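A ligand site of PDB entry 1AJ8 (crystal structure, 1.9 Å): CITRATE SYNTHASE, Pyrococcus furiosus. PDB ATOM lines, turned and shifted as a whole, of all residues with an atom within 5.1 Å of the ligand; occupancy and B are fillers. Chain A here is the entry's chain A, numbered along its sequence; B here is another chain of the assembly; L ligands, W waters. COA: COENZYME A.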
ATOM      1  N   PRO A 216     -30.491 -19.950  25.118  1.00  0.00           N
ATOM      2  CA  PRO A 216     -29.278 -19.358  25.691  1.00  0.00           C
ATOM      3  C   PRO A 216     -27.956 -19.948  25.189  1.00  0.00           C
ATOM      4  O   PRO A 216     -26.918 -19.282  25.263  1.00  0.00           O
ATOM      5  CB  PRO A 216     -29.458 -19.551  27.200  1.00  0.00           C
ATOM      6  CG  PRO A 216     -30.433 -20.656  27.328  1.00  0.00           C
ATOM      7  CD  PRO A 216     -31.358 -20.528  26.159  1.00  0.00           C
ATOM      8  N   ILE A 217     -27.966 -21.185  24.689  1.00  0.00           N
ATOM      9  CA  ILE A 217     -26.723 -21.735  24.174  1.00  0.00           C
ATOM     10  C   ILE A 217     -26.689 -21.631  22.653  1.00  0.00           C
ATOM     11  O   ILE A 217     -25.817 -22.200  22.001  1.00  0.00           O
ATOM     12  CB  ILE A 217     -26.445 -23.204  24.624  1.00  0.00           C
ATOM     13  CG1 ILE A 217     -27.567 -24.145  24.203  1.00  0.00           C
ATOM     14  CG2 ILE A 217     -26.222 -23.234  26.130  1.00  0.00           C
ATOM     15  CD1 ILE A 217     -27.197 -25.603  24.412  1.00  0.00           C
ATOM     16  N   HIS A 218     -27.666 -20.907  22.098  1.00  0.00           N
ATOM     17  CA  HIS A 218     -27.672 -20.633  20.675  1.00  0.00           C
ATOM     18  C   HIS A 218     -27.644 -19.108  20.581  1.00  0.00           C
ATOM     19  O   HIS A 218     -26.885 -18.464  21.296  1.00  0.00           O
ATOM     20  CB  HIS A 218     -28.912 -21.186  19.948  1.00  0.00           C
ATOM     21  CG  HIS A 218     -28.749 -21.201  18.457  1.00  0.00           C
ATOM     22  ND1 HIS A 218     -29.781 -21.479  17.589  1.00  0.00           N
ATOM     23  CD2 HIS A 218     -27.674 -20.937  17.674  1.00  0.00           C
ATOM     24  CE1 HIS A 218     -29.347 -21.403  16.344  1.00  0.00           C
ATOM     25  NE2 HIS A 218     -28.064 -21.077  16.370  1.00  0.00           N
ATOM     26  N   GLY A 219     -28.476 -18.513  19.737  1.00  0.00           N
ATOM     27  CA  GLY A 219     -28.475 -17.058  19.603  1.00  0.00           C
ATOM     28  C   GLY A 219     -28.669 -16.267  20.894  1.00  0.00           C
ATOM     29  O   GLY A 219     -28.188 -15.142  21.002  1.00  0.00           O
ATOM     30  N   ALA A 221     -27.216 -16.457  23.475  1.00  0.00           N
ATOM     31  CA  ALA A 221     -25.931 -16.201  24.133  1.00  0.00           C
ATOM     32  C   ALA A 221     -25.442 -14.778  23.890  1.00  0.00           C
ATOM     33  O   ALA A 221     -24.582 -14.287  24.639  1.00  0.00           O
ATOM     34  CB  ALA A 221     -24.896 -17.190  23.638  1.00  0.00           C
ATOM     35  N   LYS A 249     -18.126 -26.093  36.165  1.00  0.00           N
ATOM     36  CA  LYS A 249     -18.556 -26.657  34.894  1.00  0.00           C
ATOM     37  C   LYS A 249     -19.567 -25.724  34.246  1.00  0.00           C
ATOM     38  O   LYS A 249     -20.467 -26.167  33.543  1.00  0.00           O
ATOM     39  CB  LYS A 249     -19.188 -28.035  35.107  1.00  0.00           C
ATOM     40  CG  LYS A 249     -18.205 -29.204  35.033  1.00  0.00           C
ATOM     41  CD  LYS A 249     -18.412 -30.036  33.777  1.00  0.00           C
ATOM     42  CE  LYS A 249     -17.548 -31.296  33.793  1.00  0.00           C
ATOM     43  NZ  LYS A 249     -16.348 -31.190  32.898  1.00  0.00           N
ATOM     44  N   ARG A 250     -19.430 -24.424  34.494  1.00  0.00           N
ATOM     45  CA  ARG A 250     -20.334 -23.431  33.920  1.00  0.00           C
ATOM     46  C   ARG A 250     -19.876 -23.071  32.509  1.00  0.00           C
ATOM     47  O   ARG A 250     -18.682 -22.952  32.266  1.00  0.00           O
ATOM     48  CB  ARG A 250     -20.367 -22.161  34.762  1.00  0.00           C
ATOM     49  CG  ARG A 250     -21.469 -21.194  34.359  1.00  0.00           C
ATOM     50  CD  ARG A 250     -20.942 -19.781  34.169  1.00  0.00           C
ATOM     51  NE  ARG A 250     -20.943 -19.026  35.420  1.00  0.00           N
ATOM     52  CZ  ARG A 250     -21.554 -17.852  35.592  1.00  0.00           C
ATOM     53  NH1 ARG A 250     -22.212 -17.271  34.601  1.00  0.00           N
ATOM     54  NH2 ARG A 250     -21.485 -17.255  36.775  1.00  0.00           N
ATOM     55  N   LYS A 251     -20.816 -22.906  31.592  1.00  0.00           N
ATOM     56  CA  LYS A 251     -20.467 -22.563  30.229  1.00  0.00           C
ATOM     57  C   LYS A 251     -20.075 -21.090  30.130  1.00  0.00           C
ATOM     58  O   LYS A 251     -20.781 -20.223  30.657  1.00  0.00           O
ATOM     59  CB  LYS A 251     -21.659 -22.825  29.292  1.00  0.00           C
ATOM     60  CG  LYS A 251     -22.021 -24.291  29.118  1.00  0.00           C
ATOM     61  CD  LYS A 251     -21.062 -24.985  28.147  1.00  0.00           C
ATOM     62  CE  LYS A 251     -21.180 -26.512  28.227  1.00  0.00           C
ATOM     63  NZ  LYS A 251     -20.563 -27.045  29.480  1.00  0.00           N
ATOM     64  N   ILE A 252     -18.959 -20.797  29.479  1.00  0.00           N
ATOM     65  CA  ILE A 252     -18.558 -19.405  29.296  1.00  0.00           C
ATOM     66  C   ILE A 252     -19.327 -18.974  28.060  1.00  0.00           C
ATOM     67  O   ILE A 252     -19.098 -19.475  26.969  1.00  0.00           O
ATOM     68  CB  ILE A 252     -17.023 -19.263  29.046  1.00  0.00           C
ATOM     69  CG1 ILE A 252     -16.271 -19.382  30.372  1.00  0.00           C
ATOM     70  CG2 ILE A 252     -16.715 -17.897  28.432  1.00  0.00           C
ATOM     71  CD1 ILE A 252     -15.362 -20.578  30.455  1.00  0.00           C
ATOM     72  N   MET A 253     -20.268 -18.056  28.242  1.00  0.00           N
ATOM     73  CA  MET A 253     -21.078 -17.572  27.140  1.00  0.00           C
ATOM     74  C   MET A 253     -20.284 -16.776  26.113  1.00  0.00           C
ATOM     75  O   MET A 253     -19.478 -15.913  26.464  1.00  0.00           O
ATOM     76  CB  MET A 253     -22.237 -16.748  27.690  1.00  0.00           C
ATOM     77  CG  MET A 253     -23.235 -17.584  28.486  1.00  0.00           C
ATOM     78  SD  MET A 253     -24.322 -18.522  27.370  1.00  0.00           S
ATOM     79  CE  MET A 253     -25.052 -19.699  28.490  1.00  0.00           C
ATOM     80  N   GLY A 254     -20.518 -17.076  24.841  1.00  0.00           N
ATOM     81  CA  GLY A 254     -19.808 -16.407  23.765  1.00  0.00           C
ATOM     82  C   GLY A 254     -18.598 -17.210  23.352  1.00  0.00           C
ATOM     83  O   GLY A 254     -17.847 -16.820  22.452  1.00  0.00           O
ATOM     84  N   ALA A 255     -18.404 -18.355  24.017  1.00  0.00           N
ATOM     85  CA  ALA A 255     -17.276 -19.242  23.721  1.00  0.00           C
ATOM     86  C   ALA A 255     -17.801 -20.608  23.324  1.00  0.00           C
ATOM     87  O   ALA A 255     -18.863 -21.028  23.759  1.00  0.00           O
ATOM     88  CB  ALA A 255     -16.371 -19.367  24.927  1.00  0.00           C
ATOM     89  N   GLY A 256     -17.033 -21.311  22.485  1.00  0.00           N
ATOM     90  CA  GLY A 256     -17.427 -22.630  22.057  1.00  0.00           C
ATOM     91  C   GLY A 256     -18.246 -22.614  20.785  1.00  0.00           C
ATOM     92  O   GLY A 256     -18.957 -21.648  20.507  1.00  0.00           O
ATOM     93  N   HIS A 257     -18.128 -23.676  20.007  1.00  0.00           N
ATOM     94  CA  HIS A 257     -18.867 -23.796  18.758  1.00  0.00           C
ATOM     95  C   HIS A 257     -18.812 -25.226  18.254  1.00  0.00           C
ATOM     96  O   HIS A 257     -17.784 -25.894  18.366  1.00  0.00           O
ATOM     97  CB  HIS A 257     -18.287 -22.864  17.702  1.00  0.00           C
ATOM     98  CG  HIS A 257     -19.237 -22.564  16.576  1.00  0.00           C
ATOM     99  ND1 HIS A 257     -19.341 -23.369  15.458  1.00  0.00           N
ATOM    100  CD2 HIS A 257     -20.142 -21.580  16.419  1.00  0.00           C
ATOM    101  CE1 HIS A 257     -20.270 -22.881  14.662  1.00  0.00           C
ATOM    102  NE2 HIS A 257     -20.779 -21.797  15.224  1.00  0.00           N
ATOM    103  N   ARG A 258     -19.924 -25.705  17.700  1.00  0.00           N
ATOM    104  CA  ARG A 258     -19.964 -27.066  17.196  1.00  0.00           C
ATOM    105  C   ARG A 258     -19.017 -27.242  16.019  1.00  0.00           C
ATOM    106  O   ARG A 258     -18.374 -28.282  15.907  1.00  0.00           O
ATOM    107  CB  ARG A 258     -21.390 -27.443  16.772  1.00  0.00           C
ATOM    108  CG  ARG A 258     -21.490 -28.733  15.950  1.00  0.00           C
ATOM    109  CD  ARG A 258     -21.071 -29.961  16.756  1.00  0.00           C
ATOM    110  NE  ARG A 258     -21.805 -30.096  18.009  1.00  0.00           N
ATOM    111  CZ  ARG A 258     -22.999 -30.650  18.124  1.00  0.00           C
ATOM    112  NH1 ARG A 258     -23.608 -31.123  17.039  1.00  0.00           N
ATOM    113  NH2 ARG A 258     -23.588 -30.750  19.306  1.00  0.00           N
ATOM    114  N   LYS A 261     -13.358 -24.686  15.705  1.00  0.00           N
ATOM    115  CA  LYS A 261     -12.513 -25.197  16.779  1.00  0.00           C
ATOM    116  C   LYS A 261     -11.371 -24.207  16.934  1.00  0.00           C
ATOM    117  O   LYS A 261     -10.327 -24.511  17.501  1.00  0.00           O
ATOM    118  CB  LYS A 261     -11.989 -26.585  16.422  1.00  0.00           C
ATOM    119  CG  LYS A 261     -13.099 -27.626  16.201  1.00  0.00           C
ATOM    120  CD  LYS A 261     -13.893 -27.874  17.481  1.00  0.00           C
ATOM    121  CE  LYS A 261     -15.283 -28.422  17.196  1.00  0.00           C
ATOM    122  NZ  LYS A 261     -16.189 -28.234  18.369  1.00  0.00           N
ATOM    123  N   LEU A 297      -8.608 -23.066  27.160  1.00  0.00           N
ATOM    124  CA  LEU A 297      -9.599 -23.869  26.458  1.00  0.00           C
ATOM    125  C   LEU A 297      -9.375 -24.113  24.972  1.00  0.00           C
ATOM    126  O   LEU A 297     -10.087 -24.926  24.362  1.00  0.00           O
ATOM    127  CB  LEU A 297     -10.988 -23.250  26.682  1.00  0.00           C
ATOM    128  CG  LEU A 297     -11.355 -22.961  28.137  1.00  0.00           C
ATOM    129  CD1 LEU A 297     -12.741 -22.353  28.195  1.00  0.00           C
ATOM    130  CD2 LEU A 297     -11.301 -24.256  28.951  1.00  0.00           C
ATOM    131  N   LYS A 300      -8.776 -27.645  23.635  1.00  0.00           N
ATOM    132  CA  LYS A 300     -10.036 -28.364  23.706  1.00  0.00           C
ATOM    133  C   LYS A 300     -10.904 -28.068  22.486  1.00  0.00           C
ATOM    134  O   LYS A 300     -11.884 -28.764  22.229  1.00  0.00           O
ATOM    135  CB  LYS A 300     -10.800 -27.934  24.956  1.00  0.00           C
ATOM    136  CG  LYS A 300     -11.057 -29.021  25.946  1.00  0.00           C
ATOM    137  CD  LYS A 300     -12.035 -28.561  27.002  1.00  0.00           C
ATOM    138  CE  LYS A 300     -13.223 -29.492  27.082  1.00  0.00           C
ATOM    139  NZ  LYS A 300     -13.677 -29.673  28.479  1.00  0.00           N
ATOM    140  N   ILE A 302     -12.291 -25.018  22.094  1.00  0.00           N
ATOM    141  CA  ILE A 302     -13.231 -23.969  22.537  1.00  0.00           C
ATOM    142  C   ILE A 302     -12.603 -22.586  22.370  1.00  0.00           C
ATOM    143  O   ILE A 302     -11.671 -22.225  23.082  1.00  0.00           O
ATOM    144  CB  ILE A 302     -13.611 -24.144  24.028  1.00  0.00           C
ATOM    145  CG1 ILE A 302     -14.282 -25.489  24.250  1.00  0.00           C
ATOM    146  CG2 ILE A 302     -14.552 -23.021  24.465  1.00  0.00           C
ATOM    147  CD1 ILE A 302     -14.094 -26.006  25.638  1.00  0.00           C
ATOM    148  N   ASN A 305     -16.783 -17.201  19.953  1.00  0.00           N
ATOM    149  CA  ASN A 305     -17.740 -17.283  18.858  1.00  0.00           C
ATOM    150  C   ASN A 305     -18.429 -15.943  18.597  1.00  0.00           C
ATOM    151  O   ASN A 305     -18.253 -14.980  19.346  1.00  0.00           O
ATOM    152  CB  ASN A 305     -18.782 -18.398  19.104  1.00  0.00           C
ATOM    153  CG  ASN A 305     -19.708 -18.100  20.265  1.00  0.00           C
ATOM    154  OD1 ASN A 305     -20.283 -17.024  20.353  1.00  0.00           O
ATOM    155  ND2 ASN A 305     -19.870 -19.069  21.159  1.00  0.00           N
ATOM    156  N   ASP A 307     -21.210 -14.582  19.153  1.00  0.00           N
ATOM    157  CA  ASP A 307     -22.008 -13.897  20.153  1.00  0.00           C
ATOM    158  C   ASP A 307     -21.237 -13.291  21.326  1.00  0.00           C
ATOM    159  O   ASP A 307     -21.841 -12.715  22.238  1.00  0.00           O
ATOM    160  CB  ASP A 307     -23.093 -14.849  20.689  1.00  0.00           C
ATOM    161  CG  ASP A 307     -24.138 -15.195  19.629  1.00  0.00           C
ATOM    162  OD1 ASP A 307     -24.569 -14.281  18.878  1.00  0.00           O
ATOM    163  OD2 ASP A 307     -24.527 -16.376  19.526  1.00  0.00           O
ATOM    164  N   ARG B 348     -27.618 -31.943  24.402  1.00  0.00           N
ATOM    165  CA  ARG B 348     -26.526 -31.730  23.480  1.00  0.00           C
ATOM    166  C   ARG B 348     -27.208 -31.025  22.321  1.00  0.00           C
ATOM    167  O   ARG B 348     -28.161 -31.539  21.765  1.00  0.00           O
ATOM    168  CB  ARG B 348     -25.910 -33.042  23.011  1.00  0.00           C
ATOM    169  CG  ARG B 348     -24.777 -32.814  22.022  1.00  0.00           C
ATOM    170  CD  ARG B 348     -23.485 -33.458  22.487  1.00  0.00           C
ATOM    171  NE  ARG B 348     -22.300 -32.783  21.964  1.00  0.00           N
ATOM    172  CZ  ARG B 348     -21.578 -33.202  20.931  1.00  0.00           C
ATOM    173  NH1 ARG B 348     -21.914 -34.316  20.281  1.00  0.00           N
ATOM    174  NH2 ARG B 348     -20.511 -32.535  20.548  1.00  0.00           N
ATOM    175  N   ILE B 349     -26.726 -29.834  21.966  1.00  0.00           N
ATOM    176  CA  ILE B 349     -27.336 -29.102  20.866  1.00  0.00           C
ATOM    177  C   ILE B 349     -27.328 -29.938  19.586  1.00  0.00           C
ATOM    178  O   ILE B 349     -26.347 -30.614  19.274  1.00  0.00           O
ATOM    179  CB  ILE B 349     -26.603 -27.752  20.613  1.00  0.00           C
ATOM    180  CG1 ILE B 349     -27.495 -26.844  19.749  1.00  0.00           C
ATOM    181  CG2 ILE B 349     -25.256 -27.984  19.938  1.00  0.00           C
ATOM    182  CD1 ILE B 349     -27.173 -25.356  19.884  1.00  0.00           C
HETATM  183  N1A COA L   1     -17.445 -23.045  28.173  1.00  0.00           N
HETATM  184  C2A COA L   1     -16.869 -24.107  28.822  1.00  0.00           C
HETATM  185  N3A COA L   1     -16.766 -25.370  28.344  1.00  0.00           N
HETATM  186  C4A COA L   1     -17.310 -25.629  27.137  1.00  0.00           C
HETATM  187  C5A COA L   1     -17.944 -24.607  26.454  1.00  0.00           C
HETATM  188  C6A COA L   1     -18.037 -23.266  26.978  1.00  0.00           C
HETATM  189  N6A COA L   1     -18.693 -22.323  26.283  1.00  0.00           N
HETATM  190  N7A COA L   1     -18.436 -24.964  25.332  1.00  0.00           N
HETATM  191  C8A COA L   1     -17.969 -26.284  25.139  1.00  0.00           C
HETATM  192  N9A COA L   1     -17.419 -26.675  26.368  1.00  0.00           N
HETATM  193  C1B COA L   1     -16.879 -27.972  26.835  1.00  0.00           C
HETATM  194  C2B COA L   1     -18.015 -28.915  27.256  1.00  0.00           C
HETATM  195  O2B COA L   1     -18.494 -28.760  28.601  1.00  0.00           O
HETATM  196  C3B COA L   1     -17.445 -30.301  26.922  1.00  0.00           C
HETATM  197  O3B COA L   1     -16.530 -30.579  27.988  1.00  0.00           O
HETATM  198  P3B COA L   1     -16.140 -32.186  28.389  1.00  0.00           P
HETATM  199  O7A COA L   1     -15.497 -32.167  29.870  1.00  0.00           O
HETATM  200  O8A COA L   1     -17.505 -33.034  28.362  1.00  0.00           O
HETATM  201  O9A COA L   1     -15.101 -32.696  27.283  1.00  0.00           O
HETATM  202  C4B COA L   1     -16.538 -30.039  25.699  1.00  0.00           C
HETATM  203  O4B COA L   1     -16.195 -28.644  25.766  1.00  0.00           O
HETATM  204  C5B COA L   1     -17.249 -30.326  24.376  1.00  0.00           C
HETATM  205  O5B COA L   1     -18.270 -29.357  24.119  1.00  0.00           O
HETATM  206  P1A COA L   1     -19.834 -29.780  23.739  1.00  0.00           P
HETATM  207  O1A COA L   1     -19.950 -31.263  23.295  1.00  0.00           O
HETATM  208  O2A COA L   1     -20.848 -29.420  24.865  1.00  0.00           O
HETATM  209  O3A COA L   1     -19.995 -28.771  22.472  1.00  0.00           O
HETATM  210  P2A COA L   1     -21.222 -28.751  21.435  1.00  0.00           P
HETATM  211  O4A COA L   1     -20.678 -28.758  19.998  1.00  0.00           O
HETATM  212  O5A COA L   1     -22.210 -29.916  21.706  1.00  0.00           O
HETATM  213  O6A COA L   1     -21.915 -27.306  21.835  1.00  0.00           O
HETATM  214  CBP COA L   1     -22.141 -24.856  21.906  1.00  0.00           C
HETATM  215  CCP COA L   1     -21.622 -26.097  21.116  1.00  0.00           C
HETATM  216  CDP COA L   1     -21.892 -23.601  21.039  1.00  0.00           C
HETATM  217  CEP COA L   1     -23.673 -25.041  22.130  1.00  0.00           C
HETATM  218  CAP COA L   1     -21.349 -24.773  23.283  1.00  0.00           C
HETATM  219  OAP COA L   1     -19.945 -24.623  23.084  1.00  0.00           O
HETATM  220  C9P COA L   1     -21.901 -23.751  24.349  1.00  0.00           C
HETATM  221  O9P COA L   1     -22.838 -24.109  25.125  1.00  0.00           O
HETATM  222  N8P COA L   1     -21.362 -22.526  24.382  1.00  0.00           N
HETATM  223  C7P COA L   1     -21.812 -21.524  25.367  1.00  0.00           C
HETATM  224  C6P COA L   1     -22.972 -20.688  24.802  1.00  0.00           C
HETATM  225  C5P COA L   1     -22.554 -20.064  23.489  1.00  0.00           C
HETATM  226  O5P COA L   1     -21.883 -19.007  23.439  1.00  0.00           O
HETATM  227  N4P COA L   1     -23.157 -20.516  22.454  1.00  0.00           N
HETATM  228  C3P COA L   1     -24.198 -19.736  21.716  1.00  0.00           C
HETATM  229  O   HOH W   1     -24.402 -29.091  23.444  1.00  0.00           O
HETATM  230  O   HOH W   2     -17.860 -29.070  21.088  1.00  0.00           O
HETATM  231  O   HOH W   3     -14.533 -26.968  29.798  1.00  0.00           O
HETATM  232  O   HOH W   4     -23.439 -26.469  26.350  1.00  0.00           O
HETATM  233  O   HOH W   5     -17.189 -25.185  32.014  1.00  0.00           O
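NE of Arg 348 of chain B is in salt-bridge range of O5A of the ligand (2.9 Å).
A nitrogen (N1A) of the ligand sits at hydrogen-bond distance from the backbone NH (N) of Ile 252.
The backbone carbonyl oxygen (O) of Ile 217 sits close to a nitrogen (N4P) of the ligand (3.2 Å).
An oxygen (O2B) of the ligand lies within hydrogen-bond range of the side-chain amino group (NZ) of Lys 251 (2.8 Å).
ND2 of Asn 305 sits at hydrogen-bond distance from O5P of the ligand, 3.0 Å away.
A nitrogen (N6A) of the ligand lies within hydrogen-bond range of the backbone carbonyl oxygen of Ala 255 (2.8 Å).
The backbone NH (N) of Gly 254 is in hydrogen-bond range of an oxygen (O5P) of the ligand, 2.7 Å away.
O4A of the ligand is in salt-bridge range of NE of Arg 258 (2.6 Å).
O of Ile 252 lies within hydrogen-bond range of N6A of the ligand (3.0 Å).
NZ of Lys 300 lies within salt-bridge range of O7A of the ligand, at 3.4 Å.
The side-chain amino group (NZ) of Lys 249 is in salt-bridge range of an oxygen (O7A) of the ligand (3.3 Å).
The backbone NH of Asp 307 is in hydrogen-bond range of the side-chain amide oxygen of Asn 305 (2.9 Å).
The backbone carbonyl oxygen (O) of Gly 254 sits at hydrogen-bond distance from the backbone NH (N) of Asn 305.
NZ of Lys 261 sits at hydrogen-bond distance from O of His 257, at 2.8 Å.
The backbone NH (N) of Ile 302 sits at hydrogen-bond distance from the backbone carbonyl oxygen (O) of Leu 297 (3.2 Å).
NH2 of Arg 258 is in hydrogen-bond range of O of Ile 349 of chain B.
N of Ala 221 sits close to O of Pro 216 (3.4 Å).
ND2 of Asn 305 lies close to N of Ala 255, at 3.3 Å.
The backbone carbonyl oxygen (O) of Arg 258 sits at hydrogen-bond distance from the side-chain amino group (NZ) of Lys 261.
His 218 touches the ligand (O to C3P, 3.0 Å).
Ala 221 touches the ligand.
Met 253 touches the ligand.
Gly 256 touches the ligand (CA to OAP, 3.4 Å).
His 257 touches the ligand (N to OAP, 3.7 Å).
CD1 of Ile 302 touches O4B of the ligand (3.4 Å).
CG2 of Ile 349 of chain B touches O6A of the ligand, at 3.9 Å.
Of the 23 residues printed, 17 come within 4 Å of the ligand.
Water W2 lies within hydrogen-bond range of an oxygen (O3A) of the ligand and the side-chain amino group (NZ) of Lys 261.
Water W1 bridges N of Ile 349 of chain B and O5A of the ligand.
Water W3 lies within hydrogen-bond range of a nitrogen (N3A) of the ligand (3.1 Å) and the side-chain amino group of Lys 300 (3.1 Å).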
